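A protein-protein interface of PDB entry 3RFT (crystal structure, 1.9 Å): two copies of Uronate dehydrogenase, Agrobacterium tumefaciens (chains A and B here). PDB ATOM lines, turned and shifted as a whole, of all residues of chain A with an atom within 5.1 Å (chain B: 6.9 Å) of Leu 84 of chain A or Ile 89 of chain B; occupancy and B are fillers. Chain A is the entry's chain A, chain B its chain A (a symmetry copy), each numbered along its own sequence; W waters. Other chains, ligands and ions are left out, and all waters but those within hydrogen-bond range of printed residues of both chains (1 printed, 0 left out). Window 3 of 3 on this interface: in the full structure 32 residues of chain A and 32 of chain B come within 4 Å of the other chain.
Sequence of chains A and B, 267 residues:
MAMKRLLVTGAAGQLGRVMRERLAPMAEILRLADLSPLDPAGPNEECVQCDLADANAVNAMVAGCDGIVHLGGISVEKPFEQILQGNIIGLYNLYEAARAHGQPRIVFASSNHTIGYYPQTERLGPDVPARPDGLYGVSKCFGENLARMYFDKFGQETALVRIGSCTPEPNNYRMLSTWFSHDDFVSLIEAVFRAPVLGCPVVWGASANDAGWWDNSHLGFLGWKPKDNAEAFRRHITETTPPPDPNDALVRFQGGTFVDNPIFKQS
Of the 20 printed residues of chain B, 4 touch a printed residue of chain A. Hydrophobic or aromatic side chains of chain B that line the printed part of chain A: Leu 84, Ile 89, Tyr 92 and Phe 142. Of the 11 printed residues of chain A, 4 touch a printed residue of chain B. Hydrophobic or aromatic side chains of chain A that line the printed part of chain B: Phe 80, Leu 84, Ile 88 and Ile 89. Among the printed residues, no Asp or Glu carboxylate lies within 4 Å of a Lys or Arg side-chain nitrogen of the other chain.
Among the printed residues, pairs that only touch across the chains: Phe 80 of chain A with Tyr 92 of chain B, Leu 84 of chain A with Leu 84 of chain B, Leu 84 of chain A with Ile 89 of chain B, Ile 88 of chain A with Phe 142 of chain B and Ile 89 of chain A with Leu 84 of chain B.
Of chain A, only Leu 84 comes within 4 Å of Ile 89 of chain B. Of the printed residues of chain B, Phe 80 of chain A touches Tyr 92. Printed residues of chain B within 4 Å of Ile 88 of chain A: Phe 142 (3.9 Å). Of the printed residues of chain B, Ile 89 of chain A touches Leu 84 (3.9 Å). The nearest residue of chain B that does not touch Leu 84 of chain A is Ile 88 of chain B (4.2 Å). The nearest printed residue of chain A that does not touch Phe 142 of chain B is Phe 80 of chain A (4.2 Å).
O of Ile 83 of chain A sits at hydrogen-bond distance from N of Ile 88 of chain A (3.4 Å). O of Leu 84 of chain A sits at hydrogen-bond distance from N of Ile 89 of chain A, 2.8 Å away. The backbone carbonyl oxygen (O) of Leu 84 of chain B sits at hydrogen-bond distance from the backbone NH (N) of Ile 89 of chain B.
Leu 84 of chain B touches its own counterpart, Leu 84 of chain A. Leu 84 of chain A touches Ile 89 of chain B, and with the chains exchanged Ile 89 of chain A touches Leu 84 of chain B. 10 positions are printed for both chains. Of the 5 pairs that touch across the chains among the printed residues, 3 have their exchanged pair printed and touching as well.
Water W1 bridges OH of Tyr 92 of chain B and N of Phe 80 of chain A.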
ATOM      1  N   PHE A  80      17.559 -25.195  30.928  1.00  0.00           N
ATOM      2  CA  PHE A  80      16.713 -25.161  29.731  1.00  0.00           C
ATOM      3  C   PHE A  80      16.837 -26.426  28.884  1.00  0.00           C
ATOM      4  O   PHE A  80      15.835 -26.969  28.413  1.00  0.00           O
ATOM      5  CB  PHE A  80      17.051 -23.928  28.896  1.00  0.00           C
ATOM      6  CG  PHE A  80      16.199 -23.773  27.671  1.00  0.00           C
ATOM      7  CD1 PHE A  80      14.867 -23.416  27.781  1.00  0.00           C
ATOM      8  CD2 PHE A  80      16.733 -23.981  26.408  1.00  0.00           C
ATOM      9  CE1 PHE A  80      14.079 -23.271  26.650  1.00  0.00           C
ATOM     10  CE2 PHE A  80      15.948 -23.839  25.276  1.00  0.00           C
ATOM     11  CZ  PHE A  80      14.623 -23.481  25.400  1.00  0.00           C
ATOM     12  N   GLU A  81      18.065 -26.900  28.692  1.00  0.00           N
ATOM     13  CA  GLU A  81      18.286 -28.080  27.857  1.00  0.00           C
ATOM     14  C   GLU A  81      17.420 -29.269  28.279  1.00  0.00           C
ATOM     15  O   GLU A  81      16.838 -29.949  27.432  1.00  0.00           O
ATOM     16  CB  GLU A  81      19.766 -28.474  27.833  1.00  0.00           C
ATOM     17  CG  GLU A  81      20.669 -27.464  27.131  1.00  0.00           C
ATOM     18  CD  GLU A  81      21.162 -26.346  28.048  1.00  0.00           C
ATOM     19  OE1 GLU A  81      20.618 -26.177  29.170  1.00  0.00           O
ATOM     20  OE2 GLU A  81      22.106 -25.633  27.636  1.00  0.00           O
ATOM     21  N   GLN A  82      17.330 -29.521  29.582  1.00  0.00           N
ATOM     22  CA  GLN A  82      16.560 -30.658  30.082  1.00  0.00           C
ATOM     23  C   GLN A  82      15.059 -30.420  29.911  1.00  0.00           C
ATOM     24  O   GLN A  82      14.307 -31.321  29.534  1.00  0.00           O
ATOM     25  CB  GLN A  82      16.863 -30.913  31.556  1.00  0.00           C
ATOM     26  CG  GLN A  82      18.322 -31.235  31.855  1.00  0.00           C
ATOM     27  CD  GLN A  82      18.522 -31.607  33.307  1.00  0.00           C
ATOM     28  OE1 GLN A  82      17.694 -32.304  33.900  1.00  0.00           O
ATOM     29  NE2 GLN A  82      19.619 -31.140  33.894  1.00  0.00           N
ATOM     30  N   ILE A  83      14.629 -29.202  30.206  1.00  0.00           N
ATOM     31  CA  ILE A  83      13.210 -28.855  30.099  1.00  0.00           C
ATOM     32  C   ILE A  83      12.764 -28.897  28.634  1.00  0.00           C
ATOM     33  O   ILE A  83      11.668 -29.369  28.312  1.00  0.00           O
ATOM     34  CB  ILE A  83      12.948 -27.483  30.749  1.00  0.00           C
ATOM     35  CG1 ILE A  83      13.004 -27.631  32.276  1.00  0.00           C
ATOM     36  CG2 ILE A  83      11.604 -26.907  30.304  1.00  0.00           C
ATOM     37  CD1 ILE A  83      12.921 -26.336  33.029  1.00  0.00           C
ATOM     38  N   LEU A  84      13.635 -28.430  27.749  1.00  0.00           N
ATOM     39  CA  LEU A  84      13.372 -28.474  26.314  1.00  0.00           C
ATOM     40  C   LEU A  84      13.075 -29.899  25.845  1.00  0.00           C
ATOM     41  O   LEU A  84      12.093 -30.149  25.142  1.00  0.00           O
ATOM     42  CB  LEU A  84      14.570 -27.903  25.547  1.00  0.00           C
ATOM     43  CG  LEU A  84      14.439 -27.848  24.027  1.00  0.00           C
ATOM     44  CD1 LEU A  84      13.447 -26.764  23.652  1.00  0.00           C
ATOM     45  CD2 LEU A  84      15.796 -27.596  23.374  1.00  0.00           C
ATOM     46  N   GLN A  85      13.925 -30.842  26.236  1.00  0.00           N
ATOM     47  CA  GLN A  85      13.758 -32.236  25.826  1.00  0.00           C
ATOM     48  C   GLN A  85      12.493 -32.883  26.396  1.00  0.00           C
ATOM     49  O   GLN A  85      11.720 -33.515  25.672  1.00  0.00           O
ATOM     50  CB  GLN A  85      14.995 -33.063  26.217  1.00  0.00           C
ATOM     51  CG  GLN A  85      16.298 -32.535  25.618  1.00  0.00           C
ATOM     52  CD  GLN A  85      16.386 -32.763  24.127  1.00  0.00           C
ATOM     53  OE1 GLN A  85      15.941 -33.795  23.623  1.00  0.00           O
ATOM     54  NE2 GLN A  85      16.965 -31.802  23.407  1.00  0.00           N
ATOM     55  N   GLY A  86      12.282 -32.730  27.698  1.00  0.00           N
ATOM     56  CA  GLY A  86      11.223 -33.458  28.373  1.00  0.00           C
ATOM     57  C   GLY A  86       9.834 -32.848  28.234  1.00  0.00           C
ATOM     58  O   GLY A  86       8.846 -33.579  28.173  1.00  0.00           O
ATOM     59  N   ASN A  87       9.762 -31.520  28.184  1.00  0.00           N
ATOM     60  CA  ASN A  87       8.490 -30.802  28.327  1.00  0.00           C
ATOM     61  C   ASN A  87       8.071 -30.003  27.110  1.00  0.00           C
ATOM     62  O   ASN A  87       6.941 -29.516  27.047  1.00  0.00           O
ATOM     63  CB  ASN A  87       8.557 -29.831  29.516  1.00  0.00           C
ATOM     64  CG  ASN A  87       8.741 -30.540  30.832  1.00  0.00           C
ATOM     65  OD1 ASN A  87       8.881 -31.763  30.873  1.00  0.00           O
ATOM     66  ND2 ASN A  87       8.729 -29.775  31.924  1.00  0.00           N
ATOM     67  N   ILE A  88       8.994 -29.803  26.177  1.00  0.00           N
ATOM     68  CA  ILE A  88       8.679 -29.044  24.976  1.00  0.00           C
ATOM     69  C   ILE A  88       8.703 -29.983  23.772  1.00  0.00           C
ATOM     70  O   ILE A  88       7.660 -30.279  23.192  1.00  0.00           O
ATOM     71  CB  ILE A  88       9.609 -27.827  24.804  1.00  0.00           C
ATOM     72  CG1 ILE A  88       9.473 -26.905  26.034  1.00  0.00           C
ATOM     73  CG2 ILE A  88       9.292 -27.072  23.512  1.00  0.00           C
ATOM     74  CD1 ILE A  88      10.281 -25.635  25.960  1.00  0.00           C
ATOM     75  N   ILE A  89       9.883 -30.483  23.423  1.00  0.00           N
ATOM     76  CA  ILE A  89       9.968 -31.517  22.395  1.00  0.00           C
ATOM     77  C   ILE A  89       9.105 -32.708  22.792  1.00  0.00           C
ATOM     78  O   ILE A  89       8.357 -33.249  21.974  1.00  0.00           O
ATOM     79  CB  ILE A  89      11.434 -31.967  22.172  1.00  0.00           C
ATOM     80  CG1 ILE A  89      12.264 -30.793  21.647  1.00  0.00           C
ATOM     81  CG2 ILE A  89      11.496 -33.159  21.205  1.00  0.00           C
ATOM     82  CD1 ILE A  89      13.775 -31.054  21.654  1.00  0.00           C
ATOM     83  N   GLY A  90       9.194 -33.109  24.056  1.00  0.00           N
ATOM     84  CA  GLY A  90       8.425 -34.238  24.548  1.00  0.00           C
ATOM     85  C   GLY A  90       6.922 -34.083  24.370  1.00  0.00           C
ATOM     86  O   GLY A  90       6.220 -35.041  24.026  1.00  0.00           O
ATOM     87  N   LEU B  52      19.913 -17.742  15.586  1.00  0.00           N
ATOM     88  CA  LEU B  52      19.331 -17.519  16.913  1.00  0.00           C
ATOM     89  C   LEU B  52      19.486 -18.736  17.820  1.00  0.00           C
ATOM     90  O   LEU B  52      19.443 -18.611  19.044  1.00  0.00           O
ATOM     91  CB  LEU B  52      17.857 -17.106  16.816  1.00  0.00           C
ATOM     92  CG  LEU B  52      17.602 -15.750  16.150  1.00  0.00           C
ATOM     93  CD1 LEU B  52      16.118 -15.533  15.848  1.00  0.00           C
ATOM     94  CD2 LEU B  52      18.134 -14.610  17.006  1.00  0.00           C
ATOM     95  N   ALA B  53      19.682 -19.916  17.231  1.00  0.00           N
ATOM     96  CA  ALA B  53      19.852 -21.130  18.039  1.00  0.00           C
ATOM     97  C   ALA B  53      21.259 -21.252  18.637  1.00  0.00           C
ATOM     98  O   ALA B  53      21.513 -22.126  19.471  1.00  0.00           O
ATOM     99  CB  ALA B  53      19.507 -22.381  17.227  1.00  0.00           C
ATOM    100  N   ASP B  54      22.158 -20.377  18.201  1.00  0.00           N
ATOM    101  CA  ASP B  54      23.553 -20.371  18.657  1.00  0.00           C
ATOM    102  C   ASP B  54      23.716 -19.359  19.793  1.00  0.00           C
ATOM    103  O   ASP B  54      23.800 -18.156  19.553  1.00  0.00           O
ATOM    104  CB  ASP B  54      24.470 -20.014  17.478  1.00  0.00           C
ATOM    105  CG  ASP B  54      25.956 -20.019  17.842  1.00  0.00           C
ATOM    106  OD1 ASP B  54      26.315 -19.835  19.025  1.00  0.00           O
ATOM    107  OD2 ASP B  54      26.777 -20.193  16.918  1.00  0.00           O
ATOM    108  N   ALA B  55      23.760 -19.853  21.026  1.00  0.00           N
ATOM    109  CA  ALA B  55      23.760 -18.982  22.208  1.00  0.00           C
ATOM    110  C   ALA B  55      24.934 -18.001  22.249  1.00  0.00           C
ATOM    111  O   ALA B  55      24.764 -16.832  22.621  1.00  0.00           O
ATOM    112  CB  ALA B  55      23.707 -19.820  23.491  1.00  0.00           C
ATOM    113  N   VAL B  58      24.379 -15.325  19.678  1.00  0.00           N
ATOM    114  CA  VAL B  58      23.323 -14.439  20.151  1.00  0.00           C
ATOM    115  C   VAL B  58      23.849 -13.494  21.237  1.00  0.00           C
ATOM    116  O   VAL B  58      23.561 -12.295  21.226  1.00  0.00           O
ATOM    117  CB  VAL B  58      22.101 -15.236  20.646  1.00  0.00           C
ATOM    118  CG1 VAL B  58      21.090 -14.310  21.321  1.00  0.00           C
ATOM    119  CG2 VAL B  58      21.453 -15.958  19.464  1.00  0.00           C
ATOM    120  N   PHE B  80       7.922 -28.354  13.022  1.00  0.00           N
ATOM    121  CA  PHE B  80       8.317 -28.106  14.412  1.00  0.00           C
ATOM    122  C   PHE B  80       9.815 -27.853  14.565  1.00  0.00           C
ATOM    123  O   PHE B  80      10.231 -26.943  15.287  1.00  0.00           O
ATOM    124  CB  PHE B  80       7.886 -29.281  15.287  1.00  0.00           C
ATOM    125  CG  PHE B  80       8.198 -29.099  16.743  1.00  0.00           C
ATOM    126  CD1 PHE B  80       7.492 -28.186  17.505  1.00  0.00           C
ATOM    127  CD2 PHE B  80       9.196 -29.847  17.349  1.00  0.00           C
ATOM    128  CE1 PHE B  80       7.779 -28.018  18.851  1.00  0.00           C
ATOM    129  CE2 PHE B  80       9.487 -29.680  18.694  1.00  0.00           C
ATOM    130  CZ  PHE B  80       8.775 -28.768  19.442  1.00  0.00           C
ATOM    131  N   GLU B  81      10.630 -28.652  13.881  1.00  0.00           N
ATOM    132  CA  GLU B  81      12.081 -28.514  14.000  1.00  0.00           C
ATOM    133  C   GLU B  81      12.559 -27.084  13.744  1.00  0.00           C
ATOM    134  O   GLU B  81      13.402 -26.566  14.480  1.00  0.00           O
ATOM    135  CB  GLU B  81      12.810 -29.498  13.079  1.00  0.00           C
ATOM    136  CG  GLU B  81      12.637 -30.963  13.468  1.00  0.00           C
ATOM    137  CD  GLU B  81      11.384 -31.608  12.876  1.00  0.00           C
ATOM    138  OE1 GLU B  81      10.491 -30.880  12.370  1.00  0.00           O
ATOM    139  OE2 GLU B  81      11.299 -32.857  12.920  1.00  0.00           O
ATOM    140  N   ILE B  83      10.696 -24.249  13.810  1.00  0.00           N
ATOM    141  CA  ILE B  83      10.094 -23.335  14.782  1.00  0.00           C
ATOM    142  C   ILE B  83      10.803 -23.458  16.135  1.00  0.00           C
ATOM    143  O   ILE B  83      11.055 -22.460  16.818  1.00  0.00           O
ATOM    144  CB  ILE B  83       8.579 -23.600  14.894  1.00  0.00           C
ATOM    145  CG1 ILE B  83       7.880 -23.051  13.642  1.00  0.00           C
ATOM    146  CG2 ILE B  83       7.999 -22.976  16.162  1.00  0.00           C
ATOM    147  CD1 ILE B  83       6.421 -23.384  13.549  1.00  0.00           C
ATOM    148  N   LEU B  84      11.152 -24.685  16.497  1.00  0.00           N
ATOM    149  CA  LEU B  84      11.897 -24.942  17.727  1.00  0.00           C
ATOM    150  C   LEU B  84      13.203 -24.145  17.764  1.00  0.00           C
ATOM    151  O   LEU B  84      13.516 -23.479  18.753  1.00  0.00           O
ATOM    152  CB  LEU B  84      12.188 -26.441  17.856  1.00  0.00           C
ATOM    153  CG  LEU B  84      12.937 -26.882  19.111  1.00  0.00           C
ATOM    154  CD1 LEU B  84      12.011 -26.770  20.308  1.00  0.00           C
ATOM    155  CD2 LEU B  84      13.462 -28.307  18.958  1.00  0.00           C
ATOM    156  N   GLN B  85      13.968 -24.210  16.680  1.00  0.00           N
ATOM    157  CA  GLN B  85      15.252 -23.513  16.612  1.00  0.00           C
ATOM    158  C   GLN B  85      15.110 -21.988  16.645  1.00  0.00           C
ATOM    159  O   GLN B  85      15.796 -21.302  17.406  1.00  0.00           O
ATOM    160  CB  GLN B  85      16.031 -23.943  15.358  1.00  0.00           C
ATOM    161  CG  GLN B  85      16.294 -25.447  15.287  1.00  0.00           C
ATOM    162  CD  GLN B  85      17.310 -25.908  16.305  1.00  0.00           C
ATOM    163  OE1 GLN B  85      18.283 -25.205  16.583  1.00  0.00           O
ATOM    164  NE2 GLN B  85      17.098 -27.098  16.867  1.00  0.00           N
ATOM    165  N   GLY B  86      14.223 -21.456  15.813  1.00  0.00           N
ATOM    166  CA  GLY B  86      14.145 -20.020  15.625  1.00  0.00           C
ATOM    167  C   GLY B  86      13.358 -19.273  16.696  1.00  0.00           C
ATOM    168  O   GLY B  86      13.702 -18.140  17.033  1.00  0.00           O
ATOM    169  N   ASN B  87      12.312 -19.904  17.224  1.00  0.00           N
ATOM    170  CA  ASN B  87      11.319 -19.209  18.051  1.00  0.00           C
ATOM    171  C   ASN B  87      11.234 -19.694  19.484  1.00  0.00           C
ATOM    172  O   ASN B  87      10.574 -19.066  20.313  1.00  0.00           O
ATOM    173  CB  ASN B  87       9.919 -19.349  17.433  1.00  0.00           C
ATOM    174  CG  ASN B  87       9.814 -18.690  16.083  1.00  0.00           C
ATOM    175  OD1 ASN B  87      10.801 -18.169  15.560  1.00  0.00           O
ATOM    176  ND2 ASN B  87       8.610 -18.696  15.513  1.00  0.00           N
ATOM    177  N   ILE B  88      11.834 -20.844  19.764  1.00  0.00           N
ATOM    178  CA  ILE B  88      11.801 -21.386  21.116  1.00  0.00           C
ATOM    179  C   ILE B  88      13.208 -21.340  21.706  1.00  0.00           C
ATOM    180  O   ILE B  88      13.475 -20.559  22.619  1.00  0.00           O
ATOM    181  CB  ILE B  88      11.182 -22.797  21.153  1.00  0.00           C
ATOM    182  CG1 ILE B  88       9.744 -22.737  20.598  1.00  0.00           C
ATOM    183  CG2 ILE B  88      11.201 -23.366  22.574  1.00  0.00           C
ATOM    184  CD1 ILE B  88       8.997 -24.045  20.646  1.00  0.00           C
ATOM    185  N   ILE B  89      14.117 -22.141  21.161  1.00  0.00           N
ATOM    186  CA  ILE B  89      15.519 -22.036  21.552  1.00  0.00           C
ATOM    187  C   ILE B  89      16.013 -20.614  21.313  1.00  0.00           C
ATOM    188  O   ILE B  89      16.684 -20.025  22.164  1.00  0.00           O
ATOM    189  CB  ILE B  89      16.397 -23.046  20.771  1.00  0.00           C
ATOM    190  CG1 ILE B  89      15.977 -24.476  21.121  1.00  0.00           C
ATOM    191  CG2 ILE B  89      17.886 -22.821  21.074  1.00  0.00           C
ATOM    192  CD1 ILE B  89      16.592 -25.541  20.204  1.00  0.00           C
ATOM    193  N   GLY B  90      15.667 -20.053  20.159  1.00  0.00           N
ATOM    194  CA  GLY B  90      16.085 -18.704  19.818  1.00  0.00           C
ATOM    195  C   GLY B  90      15.650 -17.651  20.826  1.00  0.00           C
ATOM    196  O   GLY B  90      16.406 -16.727  21.147  1.00  0.00           O
ATOM    197  N   LEU B  91      14.427 -17.777  21.326  1.00  0.00           N
ATOM    198  CA  LEU B  91      13.908 -16.813  22.299  1.00  0.00           C
ATOM    199  C   LEU B  91      14.628 -16.944  23.635  1.00  0.00           C
ATOM    200  O   LEU B  91      14.957 -15.945  24.272  1.00  0.00           O
ATOM    201  CB  LEU B  91      12.395 -16.989  22.494  1.00  0.00           C
ATOM    202  CG  LEU B  91      11.542 -15.922  21.804  1.00  0.00           C
ATOM    203  CD1 LEU B  91      11.695 -14.571  22.472  1.00  0.00           C
ATOM    204  CD2 LEU B  91      11.907 -15.823  20.318  1.00  0.00           C
ATOM    205  N   TYR B  92      14.861 -18.176  24.069  1.00  0.00           N
ATOM    206  CA  TYR B  92      15.597 -18.382  25.306  1.00  0.00           C
ATOM    207  C   TYR B  92      16.985 -17.731  25.194  1.00  0.00           C
ATOM    208  O   TYR B  92      17.414 -16.992  26.087  1.00  0.00           O
ATOM    209  CB  TYR B  92      15.700 -19.871  25.650  1.00  0.00           C
ATOM    210  CG  TYR B  92      16.676 -20.139  26.768  1.00  0.00           C
ATOM    211  CD1 TYR B  92      16.338 -19.864  28.095  1.00  0.00           C
ATOM    212  CD2 TYR B  92      17.945 -20.637  26.496  1.00  0.00           C
ATOM    213  CE1 TYR B  92      17.244 -20.095  29.122  1.00  0.00           C
ATOM    214  CE2 TYR B  92      18.856 -20.871  27.511  1.00  0.00           C
ATOM    215  CZ  TYR B  92      18.501 -20.593  28.822  1.00  0.00           C
ATOM    216  OH  TYR B  92      19.401 -20.826  29.838  1.00  0.00           O
ATOM    217  N   ASN B  93      17.674 -17.986  24.086  1.00  0.00           N
ATOM    218  CA  ASN B  93      18.989 -17.389  23.864  1.00  0.00           C
ATOM    219  C   ASN B  93      18.950 -15.872  23.856  1.00  0.00           C
ATOM    220  O   ASN B  93      19.853 -15.221  24.396  1.00  0.00           O
ATOM    221  CB  ASN B  93      19.626 -17.906  22.566  1.00  0.00           C
ATOM    222  CG  ASN B  93      20.055 -19.350  22.675  1.00  0.00           C
ATOM    223  OD1 ASN B  93      20.228 -19.859  23.777  1.00  0.00           O
ATOM    224  ND2 ASN B  93      20.221 -20.024  21.535  1.00  0.00           N
ATOM    225  N   LEU B  94      17.918 -15.302  23.230  1.00  0.00           N
ATOM    226  CA  LEU B  94      17.799 -13.847  23.183  1.00  0.00           C
ATOM    227  C   LEU B  94      17.617 -13.263  24.589  1.00  0.00           C
ATOM    228  O   LEU B  94      18.263 -12.266  24.939  1.00  0.00           O
ATOM    229  CB  LEU B  94      16.637 -13.401  22.286  1.00  0.00           C
ATOM    230  CG  LEU B  94      16.504 -11.883  22.103  1.00  0.00           C
ATOM    231  CD1 LEU B  94      17.546 -11.386  21.113  1.00  0.00           C
ATOM    232  CD2 LEU B  94      15.092 -11.500  21.639  1.00  0.00           C
ATOM    233  N   PHE B 142       4.839 -18.958  23.472  1.00  0.00           N
ATOM    234  CA  PHE B 142       6.035 -19.282  24.261  1.00  0.00           C
ATOM    235  C   PHE B 142       6.872 -18.025  24.498  1.00  0.00           C
ATOM    236  O   PHE B 142       7.291 -17.751  25.626  1.00  0.00           O
ATOM    237  CB  PHE B 142       6.881 -20.373  23.584  1.00  0.00           C
ATOM    238  CG  PHE B 142       8.212 -20.615  24.265  1.00  0.00           C
ATOM    239  CD1 PHE B 142       8.322 -21.542  25.292  1.00  0.00           C
ATOM    240  CD2 PHE B 142       9.338 -19.902  23.884  1.00  0.00           C
ATOM    241  CE1 PHE B 142       9.539 -21.756  25.931  1.00  0.00           C
ATOM    242  CE2 PHE B 142      10.567 -20.112  24.521  1.00  0.00           C
ATOM    243  CZ  PHE B 142      10.660 -21.042  25.542  1.00  0.00           C
HETATM  244  O   HOH W   1      19.250 -22.903  31.477  1.00  0.00           O
